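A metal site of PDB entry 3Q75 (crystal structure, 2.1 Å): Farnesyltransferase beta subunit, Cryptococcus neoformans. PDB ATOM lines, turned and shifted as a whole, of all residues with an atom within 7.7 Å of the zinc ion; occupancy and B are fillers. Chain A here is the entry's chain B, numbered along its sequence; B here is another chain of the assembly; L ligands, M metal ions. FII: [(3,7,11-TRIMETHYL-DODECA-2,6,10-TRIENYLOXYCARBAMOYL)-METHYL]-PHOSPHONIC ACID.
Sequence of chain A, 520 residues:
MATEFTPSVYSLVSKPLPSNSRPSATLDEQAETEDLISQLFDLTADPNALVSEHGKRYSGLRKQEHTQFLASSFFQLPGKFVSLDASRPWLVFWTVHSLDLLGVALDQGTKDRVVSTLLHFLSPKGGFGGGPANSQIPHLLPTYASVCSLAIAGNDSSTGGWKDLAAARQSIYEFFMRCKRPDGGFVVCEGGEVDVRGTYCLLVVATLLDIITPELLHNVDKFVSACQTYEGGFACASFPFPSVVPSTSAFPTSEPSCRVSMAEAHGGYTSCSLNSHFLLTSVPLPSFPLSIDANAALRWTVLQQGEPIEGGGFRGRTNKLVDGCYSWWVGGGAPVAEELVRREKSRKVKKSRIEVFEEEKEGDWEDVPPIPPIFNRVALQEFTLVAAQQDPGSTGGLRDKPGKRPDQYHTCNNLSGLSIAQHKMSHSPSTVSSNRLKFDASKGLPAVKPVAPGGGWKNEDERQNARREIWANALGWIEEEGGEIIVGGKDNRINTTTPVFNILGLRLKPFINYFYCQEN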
ATOM      1  N   VAL A 322     -18.287  14.923  36.783  1.00  0.00           N
ATOM      2  CA  VAL A 322     -17.477  13.728  36.593  1.00  0.00           C
ATOM      3  C   VAL A 322     -17.358  13.418  35.103  1.00  0.00           C
ATOM      4  O   VAL A 322     -18.252  13.739  34.315  1.00  0.00           O
ATOM      5  CB  VAL A 322     -18.008  12.499  37.363  1.00  0.00           C
ATOM      6  CG1 VAL A 322     -18.001  12.764  38.868  1.00  0.00           C
ATOM      7  CG2 VAL A 322     -19.403  12.101  36.880  1.00  0.00           C
ATOM      8  N   ASP A 323     -16.245  12.796  34.718  1.00  0.00           N
ATOM      9  CA  ASP A 323     -15.907  12.580  33.320  1.00  0.00           C
ATOM     10  C   ASP A 323     -14.873  11.449  33.220  1.00  0.00           C
ATOM     11  O   ASP A 323     -13.829  11.486  33.885  1.00  0.00           O
ATOM     12  CB  ASP A 323     -15.359  13.884  32.731  1.00  0.00           C
ATOM     13  CG  ASP A 323     -14.861  13.760  31.309  1.00  0.00           C
ATOM     14  OD1 ASP A 323     -14.636  12.643  30.796  1.00  0.00           O
ATOM     15  OD2 ASP A 323     -14.659  14.817  30.684  1.00  0.00           O
ATOM     16  N   GLY A 324     -15.187  10.453  32.398  1.00  0.00           N
ATOM     17  CA  GLY A 324     -14.318   9.285  32.201  1.00  0.00           C
ATOM     18  C   GLY A 324     -12.843   9.541  31.916  1.00  0.00           C
ATOM     19  O   GLY A 324     -11.992   8.748  32.312  1.00  0.00           O
ATOM     20  N   CYS A 325     -12.531  10.640  31.231  1.00  0.00           N
ATOM     21  CA  CYS A 325     -11.115  10.920  30.908  1.00  0.00           C
ATOM     22  C   CYS A 325     -10.289  11.217  32.171  1.00  0.00           C
ATOM     23  O   CYS A 325      -9.085  10.946  32.198  1.00  0.00           O
ATOM     24  CB  CYS A 325     -10.955  12.025  29.848  1.00  0.00           C
ATOM     25  SG  CYS A 325     -11.425  13.717  30.315  1.00  0.00           S
ATOM     26  N   TYR A 326     -10.949  11.740  33.205  1.00  0.00           N
ATOM     27  CA  TYR A 326     -10.267  12.028  34.481  1.00  0.00           C
ATOM     28  C   TYR A 326      -9.895  10.772  35.274  1.00  0.00           C
ATOM     29  O   TYR A 326      -9.160  10.866  36.258  1.00  0.00           O
ATOM     30  CB  TYR A 326     -11.067  13.030  35.329  1.00  0.00           C
ATOM     31  CG  TYR A 326     -11.275  14.338  34.612  1.00  0.00           C
ATOM     32  CD1 TYR A 326     -10.185  15.045  34.094  1.00  0.00           C
ATOM     33  CD2 TYR A 326     -12.545  14.863  34.422  1.00  0.00           C
ATOM     34  CE1 TYR A 326     -10.350  16.228  33.415  1.00  0.00           C
ATOM     35  CE2 TYR A 326     -12.737  16.060  33.736  1.00  0.00           C
ATOM     36  CZ  TYR A 326     -11.624  16.742  33.232  1.00  0.00           C
ATOM     37  OH  TYR A 326     -11.770  17.922  32.559  1.00  0.00           O
ATOM     38  N   TRP A 329      -6.356  11.203  34.159  1.00  0.00           N
ATOM     39  CA  TRP A 329      -5.731  12.443  34.637  1.00  0.00           C
ATOM     40  C   TRP A 329      -5.660  12.544  36.160  1.00  0.00           C
ATOM     41  O   TRP A 329      -4.624  12.911  36.715  1.00  0.00           O
ATOM     42  CB  TRP A 329      -6.385  13.700  34.023  1.00  0.00           C
ATOM     43  CG  TRP A 329      -6.404  13.673  32.510  1.00  0.00           C
ATOM     44  CD1 TRP A 329      -7.502  13.679  31.704  1.00  0.00           C
ATOM     45  CD2 TRP A 329      -5.266  13.617  31.636  1.00  0.00           C
ATOM     46  NE1 TRP A 329      -7.132  13.638  30.390  1.00  0.00           N
ATOM     47  CE2 TRP A 329      -5.761  13.598  30.310  1.00  0.00           C
ATOM     48  CE3 TRP A 329      -3.880  13.590  31.842  1.00  0.00           C
ATOM     49  CZ2 TRP A 329      -4.914  13.555  29.196  1.00  0.00           C
ATOM     50  CZ3 TRP A 329      -3.034  13.537  30.726  1.00  0.00           C
ATOM     51  CH2 TRP A 329      -3.567  13.518  29.418  1.00  0.00           C
ATOM     52  N   ARG A 399     -16.453   6.925  26.562  1.00  0.00           N
ATOM     53  CA  ARG A 399     -16.971   8.290  26.529  1.00  0.00           C
ATOM     54  C   ARG A 399     -16.792   9.047  27.843  1.00  0.00           C
ATOM     55  O   ARG A 399     -16.456   8.464  28.875  1.00  0.00           O
ATOM     56  CB  ARG A 399     -18.468   8.264  26.178  1.00  0.00           C
ATOM     57  CG  ARG A 399     -19.184   7.065  26.780  1.00  0.00           C
ATOM     58  CD  ARG A 399     -20.422   7.418  27.549  1.00  0.00           C
ATOM     59  NE  ARG A 399     -21.632   7.139  26.786  1.00  0.00           N
ATOM     60  CZ  ARG A 399     -22.595   6.299  27.145  1.00  0.00           C
ATOM     61  NH1 ARG A 399     -22.533   5.626  28.290  1.00  0.00           N
ATOM     62  NH2 ARG A 399     -23.648   6.135  26.349  1.00  0.00           N
ATOM     63  N   ASP A 400     -17.027  10.354  27.761  1.00  0.00           N
ATOM     64  CA  ASP A 400     -17.081  11.272  28.891  1.00  0.00           C
ATOM     65  C   ASP A 400     -18.112  10.805  29.931  1.00  0.00           C
ATOM     66  O   ASP A 400     -17.751  10.445  31.062  1.00  0.00           O
ATOM     67  CB  ASP A 400     -17.402  12.690  28.346  1.00  0.00           C
ATOM     68  CG  ASP A 400     -17.810  13.691  29.429  1.00  0.00           C
ATOM     69  OD1 ASP A 400     -17.891  13.360  30.623  1.00  0.00           O
ATOM     70  OD2 ASP A 400     -18.062  14.856  29.039  1.00  0.00           O
ATOM     71  N   LYS A 401     -19.385  10.790  29.522  1.00  0.00           N
ATOM     72  CA  LYS A 401     -20.497  10.386  30.383  1.00  0.00           C
ATOM     73  C   LYS A 401     -21.679   9.955  29.498  1.00  0.00           C
ATOM     74  O   LYS A 401     -21.644  10.170  28.290  1.00  0.00           O
ATOM     75  CB  LYS A 401     -20.896  11.524  31.342  1.00  0.00           C
ATOM     76  CG  LYS A 401     -21.239  12.848  30.655  1.00  0.00           C
ATOM     77  CD  LYS A 401     -21.817  13.912  31.603  1.00  0.00           C
ATOM     78  CE  LYS A 401     -20.809  14.437  32.614  1.00  0.00           C
ATOM     79  NZ  LYS A 401     -19.633  15.117  31.983  1.00  0.00           N
ATOM     80  N   ASP A 407     -15.225   8.917  21.754  1.00  0.00           N
ATOM     81  CA  ASP A 407     -14.146   9.320  20.860  1.00  0.00           C
ATOM     82  C   ASP A 407     -12.842   8.638  21.261  1.00  0.00           C
ATOM     83  O   ASP A 407     -12.779   7.984  22.313  1.00  0.00           O
ATOM     84  CB  ASP A 407     -14.009  10.865  20.798  1.00  0.00           C
ATOM     85  CG  ASP A 407     -13.749  11.493  22.162  1.00  0.00           C
ATOM     86  OD1 ASP A 407     -13.087  10.871  23.024  1.00  0.00           O
ATOM     87  OD2 ASP A 407     -14.192  12.638  22.377  1.00  0.00           O
ATOM     88  N   TYR A 409      -9.942   9.908  22.215  1.00  0.00           N
ATOM     89  CA  TYR A 409      -9.403  10.508  23.428  1.00  0.00           C
ATOM     90  C   TYR A 409      -9.984   9.890  24.709  1.00  0.00           C
ATOM     91  O   TYR A 409      -9.245   9.508  25.615  1.00  0.00           O
ATOM     92  CB  TYR A 409      -9.624  12.028  23.407  1.00  0.00           C
ATOM     93  CG  TYR A 409      -9.450  12.696  24.759  1.00  0.00           C
ATOM     94  CD1 TYR A 409      -8.175  13.004  25.238  1.00  0.00           C
ATOM     95  CD2 TYR A 409     -10.550  13.031  25.552  1.00  0.00           C
ATOM     96  CE1 TYR A 409      -8.002  13.624  26.474  1.00  0.00           C
ATOM     97  CE2 TYR A 409     -10.381  13.649  26.798  1.00  0.00           C
ATOM     98  CZ  TYR A 409      -9.112  13.933  27.250  1.00  0.00           C
ATOM     99  OH  TYR A 409      -8.927  14.543  28.478  1.00  0.00           O
ATOM    100  N   HIS A 410     -11.319   9.778  24.767  1.00  0.00           N
ATOM    101  CA  HIS A 410     -11.982   9.201  25.929  1.00  0.00           C
ATOM    102  C   HIS A 410     -11.821   7.686  26.005  1.00  0.00           C
ATOM    103  O   HIS A 410     -11.828   7.124  27.090  1.00  0.00           O
ATOM    104  CB  HIS A 410     -13.450   9.630  26.007  1.00  0.00           C
ATOM    105  CG  HIS A 410     -13.634  11.051  26.412  1.00  0.00           C
ATOM    106  ND1 HIS A 410     -13.934  12.057  25.506  1.00  0.00           N
ATOM    107  CD2 HIS A 410     -13.504  11.662  27.611  1.00  0.00           C
ATOM    108  CE1 HIS A 410     -14.003  13.207  26.143  1.00  0.00           C
ATOM    109  NE2 HIS A 410     -13.742  13.000  27.425  1.00  0.00           N
ATOM    110  N   ASN A 413      -8.157   7.351  27.523  1.00  0.00           N
ATOM    111  CA  ASN A 413      -8.047   7.805  28.903  1.00  0.00           C
ATOM    112  C   ASN A 413      -8.938   7.066  29.904  1.00  0.00           C
ATOM    113  O   ASN A 413      -8.534   6.864  31.044  1.00  0.00           O
ATOM    114  CB  ASN A 413      -8.172   9.326  28.980  1.00  0.00           C
ATOM    115  CG  ASN A 413      -6.961  10.037  28.387  1.00  0.00           C
ATOM    116  OD1 ASN A 413      -5.867  10.005  28.961  1.00  0.00           O
ATOM    117  ND2 ASN A 413      -7.133  10.651  27.225  1.00  0.00           N
ATOM    118  N   ASN A 414     -10.132   6.637  29.477  1.00  0.00           N
ATOM    119  CA  ASN A 414     -10.944   5.697  30.269  1.00  0.00           C
ATOM    120  C   ASN A 414     -10.177   4.412  30.554  1.00  0.00           C
ATOM    121  O   ASN A 414     -10.101   3.964  31.698  1.00  0.00           O
ATOM    122  CB  ASN A 414     -12.258   5.355  29.566  1.00  0.00           C
ATOM    123  CG  ASN A 414     -13.380   6.327  29.888  1.00  0.00           C
ATOM    124  OD1 ASN A 414     -13.828   7.074  29.016  1.00  0.00           O
ATOM    125  ND2 ASN A 414     -13.837   6.321  31.121  1.00  0.00           N
ATOM    126  N   THR B   1     -19.332  20.850  23.556  1.00  0.00           N
ATOM    127  CA  THR B   1     -18.737  20.779  24.924  1.00  0.00           C
ATOM    128  C   THR B   1     -17.716  19.631  25.021  1.00  0.00           C
ATOM    129  O   THR B   1     -17.534  19.034  26.092  1.00  0.00           O
ATOM    130  CB  THR B   1     -19.833  20.606  26.011  1.00  0.00           C
ATOM    131  OG1 THR B   1     -21.050  21.225  25.576  1.00  0.00           O
ATOM    132  CG2 THR B   1     -19.402  21.234  27.340  1.00  0.00           C
ATOM    133  N   LYS B   2     -17.059  19.329  23.905  1.00  0.00           N
ATOM    134  CA  LYS B   2     -16.045  18.275  23.842  1.00  0.00           C
ATOM    135  C   LYS B   2     -14.893  18.549  24.809  1.00  0.00           C
ATOM    136  O   LYS B   2     -14.815  19.634  25.391  1.00  0.00           O
ATOM    137  CB  LYS B   2     -15.507  18.127  22.419  1.00  0.00           C
ATOM    138  CG  LYS B   2     -16.532  17.658  21.390  1.00  0.00           C
ATOM    139  CD  LYS B   2     -15.875  17.361  20.049  1.00  0.00           C
ATOM    140  CE  LYS B   2     -16.895  16.913  19.014  1.00  0.00           C
ATOM    141  NZ  LYS B   2     -16.276  16.711  17.675  1.00  0.00           N
ATOM    142  N   CYS B   3     -14.014  17.569  25.001  1.00  0.00           N
ATOM    143  CA  CYS B   3     -12.771  17.799  25.735  1.00  0.00           C
ATOM    144  C   CYS B   3     -11.649  18.220  24.784  1.00  0.00           C
ATOM    145  O   CYS B   3     -11.519  17.675  23.700  1.00  0.00           O
ATOM    146  CB  CYS B   3     -12.369  16.567  26.544  1.00  0.00           C
ATOM    147  SG  CYS B   3     -13.443  16.237  27.946  1.00  0.00           S
ATOM    148  N   VAL B   4     -10.866  19.218  25.215  1.00  0.00           N
ATOM    149  CA  VAL B   4      -9.775  19.774  24.425  1.00  0.00           C
ATOM    150  C   VAL B   4      -8.496  19.765  25.261  1.00  0.00           C
ATOM    151  O   VAL B   4      -8.483  20.280  26.381  1.00  0.00           O
ATOM    152  CB  VAL B   4     -10.105  21.224  23.925  1.00  0.00           C
ATOM    153  CG1 VAL B   4      -8.930  21.828  23.162  1.00  0.00           C
ATOM    154  CG2 VAL B   4     -11.374  21.237  23.060  1.00  0.00           C
ATOM    155  N   VAL B   5      -7.435  19.169  24.722  1.00  0.00           N
ATOM    156  CA  VAL B   5      -6.164  19.053  25.431  1.00  0.00           C
ATOM    157  C   VAL B   5      -5.053  19.790  24.700  1.00  0.00           C
ATOM    158  O   VAL B   5      -3.963  19.981  25.234  1.00  0.00           O
ATOM    159  CB  VAL B   5      -5.735  17.577  25.651  1.00  0.00           C
ATOM    160  CG1 VAL B   5      -6.777  16.829  26.458  1.00  0.00           C
ATOM    161  CG2 VAL B   5      -5.455  16.872  24.324  1.00  0.00           C
HETATM  162  C1  FII L   1      -1.753  17.337  26.534  1.00  0.00           C
HETATM  163  C2  FII L   1      -2.044  17.035  27.992  1.00  0.00           C
HETATM  164  C6  FII L   1      -1.156  16.038  28.732  1.00  0.00           C
HETATM  165  C10 FII L   1      -3.125  17.718  28.570  1.00  0.00           C
HETATM  166  C11 FII L   1      -3.683  17.683  29.838  1.00  0.00           C
HETATM  167  C12 FII L   1      -5.066  17.029  29.714  1.00  0.00           C
HETATM  168  C15 FII L   1      -6.281  17.884  30.102  1.00  0.00           C
HETATM  169  C18 FII L   1      -7.557  17.120  30.481  1.00  0.00           C
HETATM  170  C22 FII L   1      -6.268  19.282  30.122  1.00  0.00           C
HETATM  171  C23 FII L   1      -7.354  20.100  30.485  1.00  0.00           C
HETATM  172  C24 FII L   1      -7.392  21.423  29.713  1.00  0.00           C
HETATM  173  C27 FII L   1      -8.563  22.341  30.127  1.00  0.00           C
HETATM  174  C30 FII L   1      -8.666  22.854  31.570  1.00  0.00           C
HETATM  175  C34 FII L   1      -9.508  22.731  29.170  1.00  0.00           C
HETATM  176  C35 FII L   1     -10.611  23.563  29.368  1.00  0.00           C
HETATM  177  O36 FII L   1     -11.812  22.994  28.829  1.00  0.00           O
HETATM  178  N42 FII L   1     -12.194  21.834  29.437  1.00  0.00           N
HETATM  179  C43 FII L   1     -13.195  21.774  30.319  1.00  0.00           C
HETATM  180  O44 FII L   1     -13.853  22.746  30.686  1.00  0.00           O
HETATM  181  C45 FII L   1     -13.516  20.378  30.855  1.00  0.00           C
HETATM  182  P46 FII L   1     -14.119  20.400  32.578  1.00  0.00           P
HETATM  183  O49 FII L   1     -13.964  18.869  33.057  1.00  0.00           O
HETATM  184  O50 FII L   1     -13.038  21.245  33.389  1.00  0.00           O
HETATM  185  O51 FII L   1     -15.490  20.919  32.727  1.00  0.00           O
HETATM  186 ZN    ZN M   1     -13.347  14.198  29.103  1.00  0.00          ZN
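An oxygen (O49) of the ligand is in hydrogen-bond range of the side-chain hydroxyl (OH) of Tyr 326 (2.4 Å).
The side-chain hydroxyl (OH) of Tyr 409 lies close to the side-chain sulfur (SG) of Cys 325, at 3.2 Å.
The side-chain hydroxyl (OH) of Tyr 409 lies within hydrogen-bond range of the indole nitrogen (NE1) of Trp 329, 2.8 Å away.
The side-chain amide oxygen (OD1) of Asn 414 lies close to the backbone carbonyl oxygen (O) of His 410 (2.8 Å).
O of Tyr 409 lies within hydrogen-bond range of ND2 of Asn 413 (2.9 Å).
N of His 410 is in hydrogen-bond range of OD1 of Asp 407, 2.7 Å away.
The side-chain carboxylate (OD1) of Asp 407 lies close to the backbone NH (N) of Tyr 409 (3.4 Å).
CE2 of Tyr 409 touches the zinc ion (3.8 Å).
The zinc ion is bound by a ring nitrogen (NE2) of His 410 (2.1 Å).
The zinc ion is bound by OD2 of Asp 323 (2.1 Å).
SG of Cys 325 is bound to the zinc ion (2.3 Å).
The zinc ion is bound by the side-chain sulfur (SG) of Cys 3 of chain B (2.3 Å).
The zinc ion has four donor atoms within binding distance.
Slightly farther from the zinc ion lies the side-chain carboxylate (OD1) of Asp 323 (2.6 Å).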
